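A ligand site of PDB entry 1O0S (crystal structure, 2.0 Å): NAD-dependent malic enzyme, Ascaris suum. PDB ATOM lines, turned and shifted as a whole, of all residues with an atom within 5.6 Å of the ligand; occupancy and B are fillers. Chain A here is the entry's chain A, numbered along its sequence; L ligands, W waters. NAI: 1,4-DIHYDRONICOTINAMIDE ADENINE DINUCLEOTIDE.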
ATOM      1  N   ARG A 181     -21.428  24.412  -4.075  1.00  0.00           N
ATOM      2  CA  ARG A 181     -20.892  25.212  -3.000  1.00  0.00           C
ATOM      3  C   ARG A 181     -19.745  26.136  -3.394  1.00  0.00           C
ATOM      4  O   ARG A 181     -18.622  25.996  -2.903  1.00  0.00           O
ATOM      5  CB  ARG A 181     -20.437  24.309  -1.842  1.00  0.00           C
ATOM      6  CG  ARG A 181     -20.253  25.041  -0.515  1.00  0.00           C
ATOM      7  CD  ARG A 181     -19.018  24.538   0.238  1.00  0.00           C
ATOM      8  NE  ARG A 181     -17.795  24.951  -0.453  1.00  0.00           N
ATOM      9  CZ  ARG A 181     -16.573  24.844   0.048  1.00  0.00           C
ATOM     10  NH1 ARG A 181     -16.372  24.330   1.256  1.00  0.00           N
ATOM     11  NH2 ARG A 181     -15.538  25.258  -0.682  1.00  0.00           N
ATOM     12  N   LEU A 183     -17.427  28.705  -2.984  1.00  0.00           N
ATOM     13  CA  LEU A 183     -16.952  29.344  -1.754  1.00  0.00           C
ATOM     14  C   LEU A 183     -17.396  30.780  -1.510  1.00  0.00           C
ATOM     15  O   LEU A 183     -16.942  31.710  -2.176  1.00  0.00           O
ATOM     16  CB  LEU A 183     -15.421  29.288  -1.680  1.00  0.00           C
ATOM     17  CG  LEU A 183     -14.891  29.583  -0.275  1.00  0.00           C
ATOM     18  CD1 LEU A 183     -15.394  28.509   0.679  1.00  0.00           C
ATOM     19  CD2 LEU A 183     -13.375  29.607  -0.274  1.00  0.00           C
ATOM     20  N   ASN A 275     -20.132  20.550   1.223  1.00  0.00           N
ATOM     21  CA  ASN A 275     -19.299  19.894   2.232  1.00  0.00           C
ATOM     22  C   ASN A 275     -19.488  18.393   2.470  1.00  0.00           C
ATOM     23  O   ASN A 275     -18.533  17.623   2.349  1.00  0.00           O
ATOM     24  CB  ASN A 275     -19.407  20.625   3.575  1.00  0.00           C
ATOM     25  CG  ASN A 275     -18.715  21.966   3.568  1.00  0.00           C
ATOM     26  OD1 ASN A 275     -17.738  22.169   2.844  1.00  0.00           O
ATOM     27  ND2 ASN A 275     -19.206  22.895   4.398  1.00  0.00           N
ATOM     28  N   ASP A 294      -9.324  19.832  -2.966  1.00  0.00           N
ATOM     29  CA  ASP A 294      -8.590  20.934  -2.374  1.00  0.00           C
ATOM     30  C   ASP A 294      -9.256  21.567  -1.148  1.00  0.00           C
ATOM     31  O   ASP A 294      -8.574  21.931  -0.194  1.00  0.00           O
ATOM     32  CB  ASP A 294      -8.331  22.024  -3.414  1.00  0.00           C
ATOM     33  CG  ASP A 294      -7.464  23.135  -2.883  1.00  0.00           C
ATOM     34  OD1 ASP A 294      -6.283  22.870  -2.582  1.00  0.00           O
ATOM     35  OD2 ASP A 294      -7.958  24.284  -2.745  1.00  0.00           O
ATOM     36  N   ASP A 295     -10.582  21.709  -1.189  1.00  0.00           N
ATOM     37  CA  ASP A 295     -11.317  22.321  -0.072  1.00  0.00           C
ATOM     38  C   ASP A 295     -11.087  21.573   1.223  1.00  0.00           C
ATOM     39  O   ASP A 295     -10.978  22.187   2.290  1.00  0.00           O
ATOM     40  CB  ASP A 295     -12.820  22.364  -0.379  1.00  0.00           C
ATOM     41  CG  ASP A 295     -13.145  23.307  -1.523  1.00  0.00           C
ATOM     42  OD1 ASP A 295     -12.749  24.490  -1.433  1.00  0.00           O
ATOM     43  OD2 ASP A 295     -13.770  22.867  -2.507  1.00  0.00           O
ATOM     44  N   THR A 299      -6.995  22.644   2.271  1.00  0.00           N
ATOM     45  CA  THR A 299      -7.175  23.554   3.398  1.00  0.00           C
ATOM     46  C   THR A 299      -6.448  22.987   4.624  1.00  0.00           C
ATOM     47  O   THR A 299      -5.586  23.653   5.211  1.00  0.00           O
ATOM     48  CB  THR A 299      -8.670  23.707   3.726  1.00  0.00           C
ATOM     49  OG1 THR A 299      -9.355  24.212   2.567  1.00  0.00           O
ATOM     50  CG2 THR A 299      -8.859  24.682   4.891  1.00  0.00           C
ATOM     51  N   PHE A 326     -12.374  27.048  17.190  1.00  0.00           N
ATOM     52  CA  PHE A 326     -13.663  27.700  17.429  1.00  0.00           C
ATOM     53  C   PHE A 326     -14.447  27.420  16.146  1.00  0.00           C
ATOM     54  O   PHE A 326     -14.251  28.097  15.127  1.00  0.00           O
ATOM     55  CB  PHE A 326     -13.500  29.206  17.631  1.00  0.00           C
ATOM     56  CG  PHE A 326     -14.772  29.896  18.004  1.00  0.00           C
ATOM     57  CD1 PHE A 326     -15.439  29.560  19.180  1.00  0.00           C
ATOM     58  CD2 PHE A 326     -15.312  30.866  17.180  1.00  0.00           C
ATOM     59  CE1 PHE A 326     -16.644  30.176  19.521  1.00  0.00           C
ATOM     60  CE2 PHE A 326     -16.522  31.493  17.513  1.00  0.00           C
ATOM     61  CZ  PHE A 326     -17.185  31.147  18.698  1.00  0.00           C
ATOM     62  N   GLY A 327     -15.320  26.424  16.192  1.00  0.00           N
ATOM     63  CA  GLY A 327     -16.063  26.035  15.014  1.00  0.00           C
ATOM     64  C   GLY A 327     -15.573  24.641  14.691  1.00  0.00           C
ATOM     65  O   GLY A 327     -14.383  24.361  14.814  1.00  0.00           O
ATOM     66  N   ALA A 328     -16.478  23.754  14.270  1.00  0.00           N
ATOM     67  CA  ALA A 328     -16.087  22.386  13.963  1.00  0.00           C
ATOM     68  C   ALA A 328     -16.760  21.838  12.713  1.00  0.00           C
ATOM     69  O   ALA A 328     -17.203  20.685  12.688  1.00  0.00           O
ATOM     70  CB  ALA A 328     -16.387  21.492  15.162  1.00  0.00           C
ATOM     71  N   GLY A 329     -16.820  22.655  11.662  1.00  0.00           N
ATOM     72  CA  GLY A 329     -17.443  22.200  10.419  1.00  0.00           C
ATOM     73  C   GLY A 329     -16.456  21.453   9.521  1.00  0.00           C
ATOM     74  O   GLY A 329     -15.677  20.620   9.992  1.00  0.00           O
ATOM     75  N   ALA A 330     -16.483  21.763   8.224  1.00  0.00           N
ATOM     76  CA  ALA A 330     -15.594  21.080   7.292  1.00  0.00           C
ATOM     77  C   ALA A 330     -14.128  21.479   7.491  1.00  0.00           C
ATOM     78  O   ALA A 330     -13.276  20.630   7.686  1.00  0.00           O
ATOM     79  CB  ALA A 330     -16.008  21.387   5.859  1.00  0.00           C
ATOM     80  N   ALA A 331     -13.863  22.782   7.466  1.00  0.00           N
ATOM     81  CA  ALA A 331     -12.497  23.278   7.614  1.00  0.00           C
ATOM     82  C   ALA A 331     -11.813  22.797   8.898  1.00  0.00           C
ATOM     83  O   ALA A 331     -10.798  22.085   8.840  1.00  0.00           O
ATOM     84  CB  ALA A 331     -12.494  24.800   7.576  1.00  0.00           C
ATOM     85  N   SER A 332     -12.366  23.179  10.037  1.00  0.00           N
ATOM     86  CA  SER A 332     -11.792  22.796  11.324  1.00  0.00           C
ATOM     87  C   SER A 332     -11.589  21.289  11.460  1.00  0.00           C
ATOM     88  O   SER A 332     -10.516  20.847  11.875  1.00  0.00           O
ATOM     89  CB  SER A 332     -12.670  23.295  12.475  1.00  0.00           C
ATOM     90  OG  SER A 332     -12.578  24.714  12.583  1.00  0.00           O
ATOM     91  N   MET A 360     -14.980  23.281  19.363  1.00  0.00           N
ATOM     92  CA  MET A 360     -16.155  24.025  19.810  1.00  0.00           C
ATOM     93  C   MET A 360     -16.977  24.302  18.561  1.00  0.00           C
ATOM     94  O   MET A 360     -16.412  24.606  17.509  1.00  0.00           O
ATOM     95  CB  MET A 360     -15.776  25.369  20.432  1.00  0.00           C
ATOM     96  CG  MET A 360     -15.136  25.311  21.803  1.00  0.00           C
ATOM     97  SD  MET A 360     -15.307  26.922  22.616  1.00  0.00           S
ATOM     98  CE  MET A 360     -13.816  27.716  22.183  1.00  0.00           C
ATOM     99  N   ASP A 361     -18.296  24.176  18.661  1.00  0.00           N
ATOM    100  CA  ASP A 361     -19.181  24.463  17.530  1.00  0.00           C
ATOM    101  C   ASP A 361     -20.313  25.356  18.021  1.00  0.00           C
ATOM    102  O   ASP A 361     -20.293  25.814  19.167  1.00  0.00           O
ATOM    103  CB  ASP A 361     -19.732  23.156  16.941  1.00  0.00           C
ATOM    104  CG  ASP A 361     -20.816  22.538  17.779  1.00  0.00           C
ATOM    105  OD1 ASP A 361     -20.903  22.857  18.989  1.00  0.00           O
ATOM    106  OD2 ASP A 361     -21.585  21.722  17.239  1.00  0.00           O
ATOM    107  N   ILE A 362     -21.293  25.623  17.168  1.00  0.00           N
ATOM    108  CA  ILE A 362     -22.401  26.496  17.549  1.00  0.00           C
ATOM    109  C   ILE A 362     -23.039  26.144  18.893  1.00  0.00           C
ATOM    110  O   ILE A 362     -23.632  27.000  19.545  1.00  0.00           O
ATOM    111  CB  ILE A 362     -23.497  26.498  16.454  1.00  0.00           C
ATOM    112  CG1 ILE A 362     -24.473  27.648  16.715  1.00  0.00           C
ATOM    113  CG2 ILE A 362     -24.236  25.167  16.452  1.00  0.00           C
ATOM    114  CD1 ILE A 362     -25.342  27.988  15.523  1.00  0.00           C
ATOM    115  N   ASP A 363     -22.925  24.885  19.328  1.00  0.00           N
ATOM    116  CA  ASP A 363     -23.499  24.476  20.601  1.00  0.00           C
ATOM    117  C   ASP A 363     -22.512  24.646  21.756  1.00  0.00           C
ATOM    118  O   ASP A 363     -22.902  24.607  22.924  1.00  0.00           O
ATOM    119  CB  ASP A 363     -23.951  23.015  20.542  1.00  0.00           C
ATOM    120  CG  ASP A 363     -25.099  22.800  19.575  1.00  0.00           C
ATOM    121  OD1 ASP A 363     -26.050  23.604  19.605  1.00  0.00           O
ATOM    122  OD2 ASP A 363     -25.036  21.821  18.809  1.00  0.00           O
ATOM    123  N   HIS A 377     -16.188  13.492  14.952  1.00  0.00           N
ATOM    124  CA  HIS A 377     -15.946  14.219  16.192  1.00  0.00           C
ATOM    125  C   HIS A 377     -15.798  13.259  17.375  1.00  0.00           C
ATOM    126  O   HIS A 377     -15.268  13.635  18.427  1.00  0.00           O
ATOM    127  CB  HIS A 377     -17.090  15.205  16.447  1.00  0.00           C
ATOM    128  CG  HIS A 377     -17.023  16.441  15.587  1.00  0.00           C
ATOM    129  ND1 HIS A 377     -18.111  17.264  15.393  1.00  0.00           N
ATOM    130  CD2 HIS A 377     -16.004  16.991  14.903  1.00  0.00           C
ATOM    131  CE1 HIS A 377     -17.754  18.278  14.623  1.00  0.00           C
ATOM    132  NE2 HIS A 377     -16.481  18.141  14.317  1.00  0.00           N
ATOM    133  N   ALA A 405     -12.656  28.772  12.610  1.00  0.00           N
ATOM    134  CA  ALA A 405     -13.240  28.439  11.307  1.00  0.00           C
ATOM    135  C   ALA A 405     -14.753  28.393  11.540  1.00  0.00           C
ATOM    136  O   ALA A 405     -15.425  27.375  11.353  1.00  0.00           O
ATOM    137  CB  ALA A 405     -12.720  27.085  10.826  1.00  0.00           C
ATOM    138  N   SER A 406     -15.260  29.534  12.010  1.00  0.00           N
ATOM    139  CA  SER A 406     -16.681  29.733  12.294  1.00  0.00           C
ATOM    140  C   SER A 406     -17.016  31.098  11.754  1.00  0.00           C
ATOM    141  O   SER A 406     -16.488  32.116  12.212  1.00  0.00           O
ATOM    142  CB  SER A 406     -16.926  29.733  13.803  1.00  0.00           C
ATOM    143  OG  SER A 406     -16.401  30.923  14.368  1.00  0.00           O
ATOM    144  N   THR A 407     -17.908  31.143  10.780  1.00  0.00           N
ATOM    145  CA  THR A 407     -18.333  32.375  10.138  1.00  0.00           C
ATOM    146  C   THR A 407     -18.706  33.559  11.054  1.00  0.00           C
ATOM    147  O   THR A 407     -19.273  34.547  10.578  1.00  0.00           O
ATOM    148  CB  THR A 407     -19.525  32.099   9.237  1.00  0.00           C
ATOM    149  OG1 THR A 407     -20.514  31.380   9.993  1.00  0.00           O
ATOM    150  CG2 THR A 407     -19.100  31.280   8.030  1.00  0.00           C
ATOM    151  N   VAL A 408     -18.385  33.488  12.343  1.00  0.00           N
ATOM    152  CA  VAL A 408     -18.723  34.553  13.273  1.00  0.00           C
ATOM    153  C   VAL A 408     -17.710  35.688  13.370  1.00  0.00           C
ATOM    154  O   VAL A 408     -16.611  35.515  13.904  1.00  0.00           O
ATOM    155  CB  VAL A 408     -18.951  33.989  14.689  1.00  0.00           C
ATOM    156  CG1 VAL A 408     -20.042  32.952  14.649  1.00  0.00           C
ATOM    157  CG2 VAL A 408     -17.681  33.363  15.198  1.00  0.00           C
ATOM    158  N   LEU A 432      -9.598  32.163  10.343  1.00  0.00           N
ATOM    159  CA  LEU A 432      -9.777  31.656   8.982  1.00  0.00           C
ATOM    160  C   LEU A 432     -11.071  31.956   8.236  1.00  0.00           C
ATOM    161  O   LEU A 432     -11.113  31.835   7.020  1.00  0.00           O
ATOM    162  CB  LEU A 432      -9.544  30.133   8.986  1.00  0.00           C
ATOM    163  CG  LEU A 432      -8.097  29.617   9.020  1.00  0.00           C
ATOM    164  CD1 LEU A 432      -7.178  30.592   9.723  1.00  0.00           C
ATOM    165  CD2 LEU A 432      -8.061  28.253   9.701  1.00  0.00           C
ATOM    166  N   SER A 433     -12.126  32.339   8.945  1.00  0.00           N
ATOM    167  CA  SER A 433     -13.385  32.630   8.251  1.00  0.00           C
ATOM    168  C   SER A 433     -13.199  33.687   7.174  1.00  0.00           C
ATOM    169  O   SER A 433     -12.461  34.650   7.351  1.00  0.00           O
ATOM    170  CB  SER A 433     -14.450  33.075   9.246  1.00  0.00           C
ATOM    171  OG  SER A 433     -14.867  31.982  10.033  1.00  0.00           O
ATOM    172  N   ASN A 434     -13.876  33.483   6.047  1.00  0.00           N
ATOM    173  CA  ASN A 434     -13.791  34.400   4.909  1.00  0.00           C
ATOM    174  C   ASN A 434     -15.150  35.042   4.649  1.00  0.00           C
ATOM    175  O   ASN A 434     -16.186  34.450   4.943  1.00  0.00           O
ATOM    176  CB  ASN A 434     -13.350  33.642   3.662  1.00  0.00           C
ATOM    177  CG  ASN A 434     -12.028  32.896   3.860  1.00  0.00           C
ATOM    178  OD1 ASN A 434     -10.983  33.502   4.081  1.00  0.00           O
ATOM    179  ND2 ASN A 434     -12.078  31.576   3.782  1.00  0.00           N
ATOM    180  N   PRO A 435     -15.172  36.274   4.119  1.00  0.00           N
ATOM    181  CA  PRO A 435     -13.990  37.083   3.789  1.00  0.00           C
ATOM    182  C   PRO A 435     -13.511  37.746   5.073  1.00  0.00           C
ATOM    183  O   PRO A 435     -13.886  37.316   6.164  1.00  0.00           O
ATOM    184  CB  PRO A 435     -14.531  38.118   2.796  1.00  0.00           C
ATOM    185  CG  PRO A 435     -15.827  37.531   2.306  1.00  0.00           C
ATOM    186  CD  PRO A 435     -16.386  36.872   3.533  1.00  0.00           C
ATOM    187  N   LYS A 438     -15.720  38.450   7.960  1.00  0.00           N
ATOM    188  CA  LYS A 438     -16.210  37.371   8.818  1.00  0.00           C
ATOM    189  C   LYS A 438     -15.112  36.883   9.748  1.00  0.00           C
ATOM    190  O   LYS A 438     -15.331  36.014  10.612  1.00  0.00           O
ATOM    191  CB  LYS A 438     -16.732  36.198   7.986  1.00  0.00           C
ATOM    192  CG  LYS A 438     -17.754  36.577   6.925  1.00  0.00           C
ATOM    193  CD  LYS A 438     -18.902  37.360   7.504  1.00  0.00           C
ATOM    194  CE  LYS A 438     -19.766  37.949   6.404  1.00  0.00           C
ATOM    195  NZ  LYS A 438     -20.784  38.892   6.955  1.00  0.00           N
ATOM    196  N   GLY A 459      -7.608  33.768   6.824  1.00  0.00           N
ATOM    197  CA  GLY A 459      -8.064  33.199   5.574  1.00  0.00           C
ATOM    198  C   GLY A 459      -8.029  34.280   4.513  1.00  0.00           C
ATOM    199  O   GLY A 459      -7.652  34.033   3.365  1.00  0.00           O
ATOM    200  N   GLY A 477      -3.531  31.936   4.995  1.00  0.00           N
ATOM    201  CA  GLY A 477      -3.437  30.495   4.843  1.00  0.00           C
ATOM    202  C   GLY A 477      -4.079  30.098   3.527  1.00  0.00           C
ATOM    203  O   GLY A 477      -5.105  29.409   3.490  1.00  0.00           O
ATOM    204  N   ASN A 479      -4.659  28.184   0.092  1.00  0.00           N
ATOM    205  CA  ASN A 479      -4.506  26.835  -0.468  1.00  0.00           C
ATOM    206  C   ASN A 479      -3.532  26.828  -1.631  1.00  0.00           C
ATOM    207  O   ASN A 479      -2.901  25.805  -1.914  1.00  0.00           O
ATOM    208  CB  ASN A 479      -5.866  26.303  -0.939  1.00  0.00           C
ATOM    209  CG  ASN A 479      -6.717  25.802   0.205  1.00  0.00           C
ATOM    210  OD1 ASN A 479      -6.483  26.144   1.363  1.00  0.00           O
ATOM    211  ND2 ASN A 479      -7.712  24.982  -0.107  1.00  0.00           N
HETATM  212  PA  NAI L   1     -19.155  24.714   8.112  1.00  0.00           P
HETATM  213  O1A NAI L   1     -20.732  24.965   7.972  1.00  0.00           O
HETATM  214  O2A NAI L   1     -18.814  23.256   7.550  1.00  0.00           O
HETATM  215  O5B NAI L   1     -18.712  24.805   9.644  1.00  0.00           O
HETATM  216  C5B NAI L   1     -18.954  25.934  10.505  1.00  0.00           C
HETATM  217  C4B NAI L   1     -18.752  25.481  11.944  1.00  0.00           C
HETATM  218  O4B NAI L   1     -18.771  26.605  12.856  1.00  0.00           O
HETATM  219  C3B NAI L   1     -19.823  24.495  12.470  1.00  0.00           C
HETATM  220  O3B NAI L   1     -19.212  23.491  13.285  1.00  0.00           O
HETATM  221  C2B NAI L   1     -20.747  25.396  13.264  1.00  0.00           C
HETATM  222  O2B NAI L   1     -21.510  24.654  14.213  1.00  0.00           O
HETATM  223  C1B NAI L   1     -19.750  26.362  13.876  1.00  0.00           C
HETATM  224  N9A NAI L   1     -20.396  27.637  14.256  1.00  0.00           N
HETATM  225  C8A NAI L   1     -21.276  28.529  13.628  1.00  0.00           C
HETATM  226  N7A NAI L   1     -21.728  29.677  14.220  1.00  0.00           N
HETATM  227  C5A NAI L   1     -21.049  29.559  15.495  1.00  0.00           C
HETATM  228  C6A NAI L   1     -20.957  30.421  16.699  1.00  0.00           C
HETATM  229  N6A NAI L   1     -21.595  31.485  16.894  1.00  0.00           N
HETATM  230  N1A NAI L   1     -20.200  29.994  17.796  1.00  0.00           N
HETATM  231  C2A NAI L   1     -19.385  28.811  17.786  1.00  0.00           C
HETATM  232  N3A NAI L   1     -19.317  27.881  16.756  1.00  0.00           N
HETATM  233  C4A NAI L   1     -20.190  28.294  15.489  1.00  0.00           C
HETATM  234  O3  NAI L   1     -18.396  25.820   7.307  1.00  0.00           O
HETATM  235  PN  NAI L   1     -16.966  25.457   6.802  1.00  0.00           P
HETATM  236  O1N NAI L   1     -17.061  24.718   5.392  1.00  0.00           O
HETATM  237  O2N NAI L   1     -16.195  24.502   7.841  1.00  0.00           O
HETATM  238  O5D NAI L   1     -16.160  26.823   6.668  1.00  0.00           O
HETATM  239  C5D NAI L   1     -15.907  27.669   7.813  1.00  0.00           C
HETATM  240  C4D NAI L   1     -15.095  28.905   7.429  1.00  0.00           C
HETATM  241  O4D NAI L   1     -13.798  28.498   6.941  1.00  0.00           O
HETATM  242  C3D NAI L   1     -15.734  29.788   6.323  1.00  0.00           C
HETATM  243  O3D NAI L   1     -15.931  31.146   6.739  1.00  0.00           O
HETATM  244  C2D NAI L   1     -14.784  29.613   5.130  1.00  0.00           C
HETATM  245  O2D NAI L   1     -14.765  30.763   4.285  1.00  0.00           O
HETATM  246  C1D NAI L   1     -13.440  29.322   5.825  1.00  0.00           C
HETATM  247  N1N NAI L   1     -12.462  28.595   4.909  1.00  0.00           N
HETATM  248  C2N NAI L   1     -12.903  27.753   3.932  1.00  0.00           C
HETATM  249  C3N NAI L   1     -12.032  27.058   3.054  1.00  0.00           C
HETATM  250  C7N NAI L   1     -12.491  26.114   1.959  1.00  0.00           C
HETATM  251  O7N NAI L   1     -13.594  25.546   1.961  1.00  0.00           O
HETATM  252  N7N NAI L   1     -11.743  25.851   0.899  1.00  0.00           N
HETATM  253  C4N NAI L   1     -10.637  27.286   3.245  1.00  0.00           C
HETATM  254  C5N NAI L   1     -10.173  28.158   4.271  1.00  0.00           C
HETATM  255  C6N NAI L   1     -11.138  28.798   5.083  1.00  0.00           C
HETATM  256  O   HOH W   1      -7.203  28.155   3.408  1.00  0.00           O
HETATM  257  O   HOH W   2     -14.816  23.803   4.075  1.00  0.00           O
HETATM  258  O   HOH W   3     -21.869  23.768   5.880  1.00  0.00           O
HETATM  259  O   HOH W   4     -15.044  24.777  10.316  1.00  0.00           O
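The backbone NH (N) of Ala 328 is in hydrogen-bond range of an oxygen (O3B) of the ligand (2.9 Å).
A nitrogen (N3A) of the ligand sits at hydrogen-bond distance from the backbone NH (N) of Ile 362.
N7N of the ligand lies within hydrogen-bond range of OG1 of Thr 299 (3.3 Å).
ND2 of Asn 275 is in hydrogen-bond range of O1N of the ligand, at 3.0 Å.
The side-chain carboxylate (OD1) of Asp 295 sits at hydrogen-bond distance from a nitrogen (N7N) of the ligand (2.9 Å).
N of Ala 331 sits at hydrogen-bond distance from O2N of the ligand, 2.9 Å away.
The side-chain amide nitrogen (ND2) of Asn 434 lies within hydrogen-bond range of an oxygen (O2D) of the ligand (2.9 Å).
The backbone NH of Asn 434 lies within hydrogen-bond range of an oxygen (O3D) of the ligand (3.2 Å).
The backbone NH (N) of Ala 330 lies within hydrogen-bond range of an oxygen (O2N) of the ligand (2.8 Å).
NH1 of Arg 181 sits at hydrogen-bond distance from O7N of the ligand, at 3.1 Å.
The backbone NH of Gly 329 is in hydrogen-bond range of an oxygen (O3B) of the ligand.
OG1 of Thr 299 is in hydrogen-bond range of O of Asp 295.
A ring nitrogen (NE2) of His 377 sits at hydrogen-bond distance from the backbone carbonyl oxygen (O) of Ala 328 (3.1 Å).
N of Ala 328 sits at hydrogen-bond distance from O of Met 360 (3.3 Å).
The side-chain hydroxyl (OG) of Ser 433 is in hydrogen-bond range of the backbone NH (N) of Thr 407, at 3.2 Å.
The backbone carbonyl oxygen of Ser 406 sits at hydrogen-bond distance from the side-chain hydroxyl of Ser 433 (2.7 Å).
O of Gly 327 is in hydrogen-bond range of OG of Ser 332, 2.9 Å away.
The side-chain amide oxygen of Asn 434 lies close to the backbone carbonyl oxygen of Gly 459, 3.4 Å away.
The backbone carbonyl oxygen (O) of Asp 294 sits at hydrogen-bond distance from the backbone NH (N) of Thr 299.
The backbone carbonyl oxygen (O) of Asp 361 lies close to a nitrogen (N3A) of the ligand.
Leu 183 touches the ligand.
Phe 326 touches the ligand.
Gly 327 touches the ligand (CA to O4B, 3.5 Å).
O of Ala 405 touches C5D of the ligand (3.6 Å).
Ser 406 touches the ligand.
CG2 of Thr 407 touches O3D of the ligand, 3.4 Å away.
Val 408 touches the ligand (CG1 to N6A, 3.1 Å).
O of Leu 432 touches C6N of the ligand (3.6 Å).
Ser 433 touches the ligand (CA to O3D, 3.3 Å).
Hydrophobic or aromatic side chains within 4 Å of the ligand: Leu 183, Phe 326, Ala 328, Ala 330, Ala 331, Ile 362 and Val 408.
Of the 30 residues printed, 20 come within 4 Å of the ligand.
The nearest printed residue that does not touch the ligand is Asn 479 (4.2 Å).
Water W3 lies within hydrogen-bond range of an oxygen (O1A) of the ligand and the side-chain amide nitrogen (ND2) of Asn 275.
Water W4 lies within hydrogen-bond range of an oxygen (O2N) of the ligand (2.7 Å), the backbone carbonyl oxygen (O) of Ala 405 (2.8 Å), the backbone NH (N) of Gly 329 (3.1 Å) and the backbone NH (N) of Ser 332 (3.1 Å).
Water W2 lies within hydrogen-bond range of an oxygen (O1N) of the ligand and the guanidinium group (NH1) of Arg 181.
Water W1 lies within hydrogen-bond range of the backbone carbonyl oxygen (O) of Gly 477 and the side-chain amide oxygen (OD1) of Asn 479.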
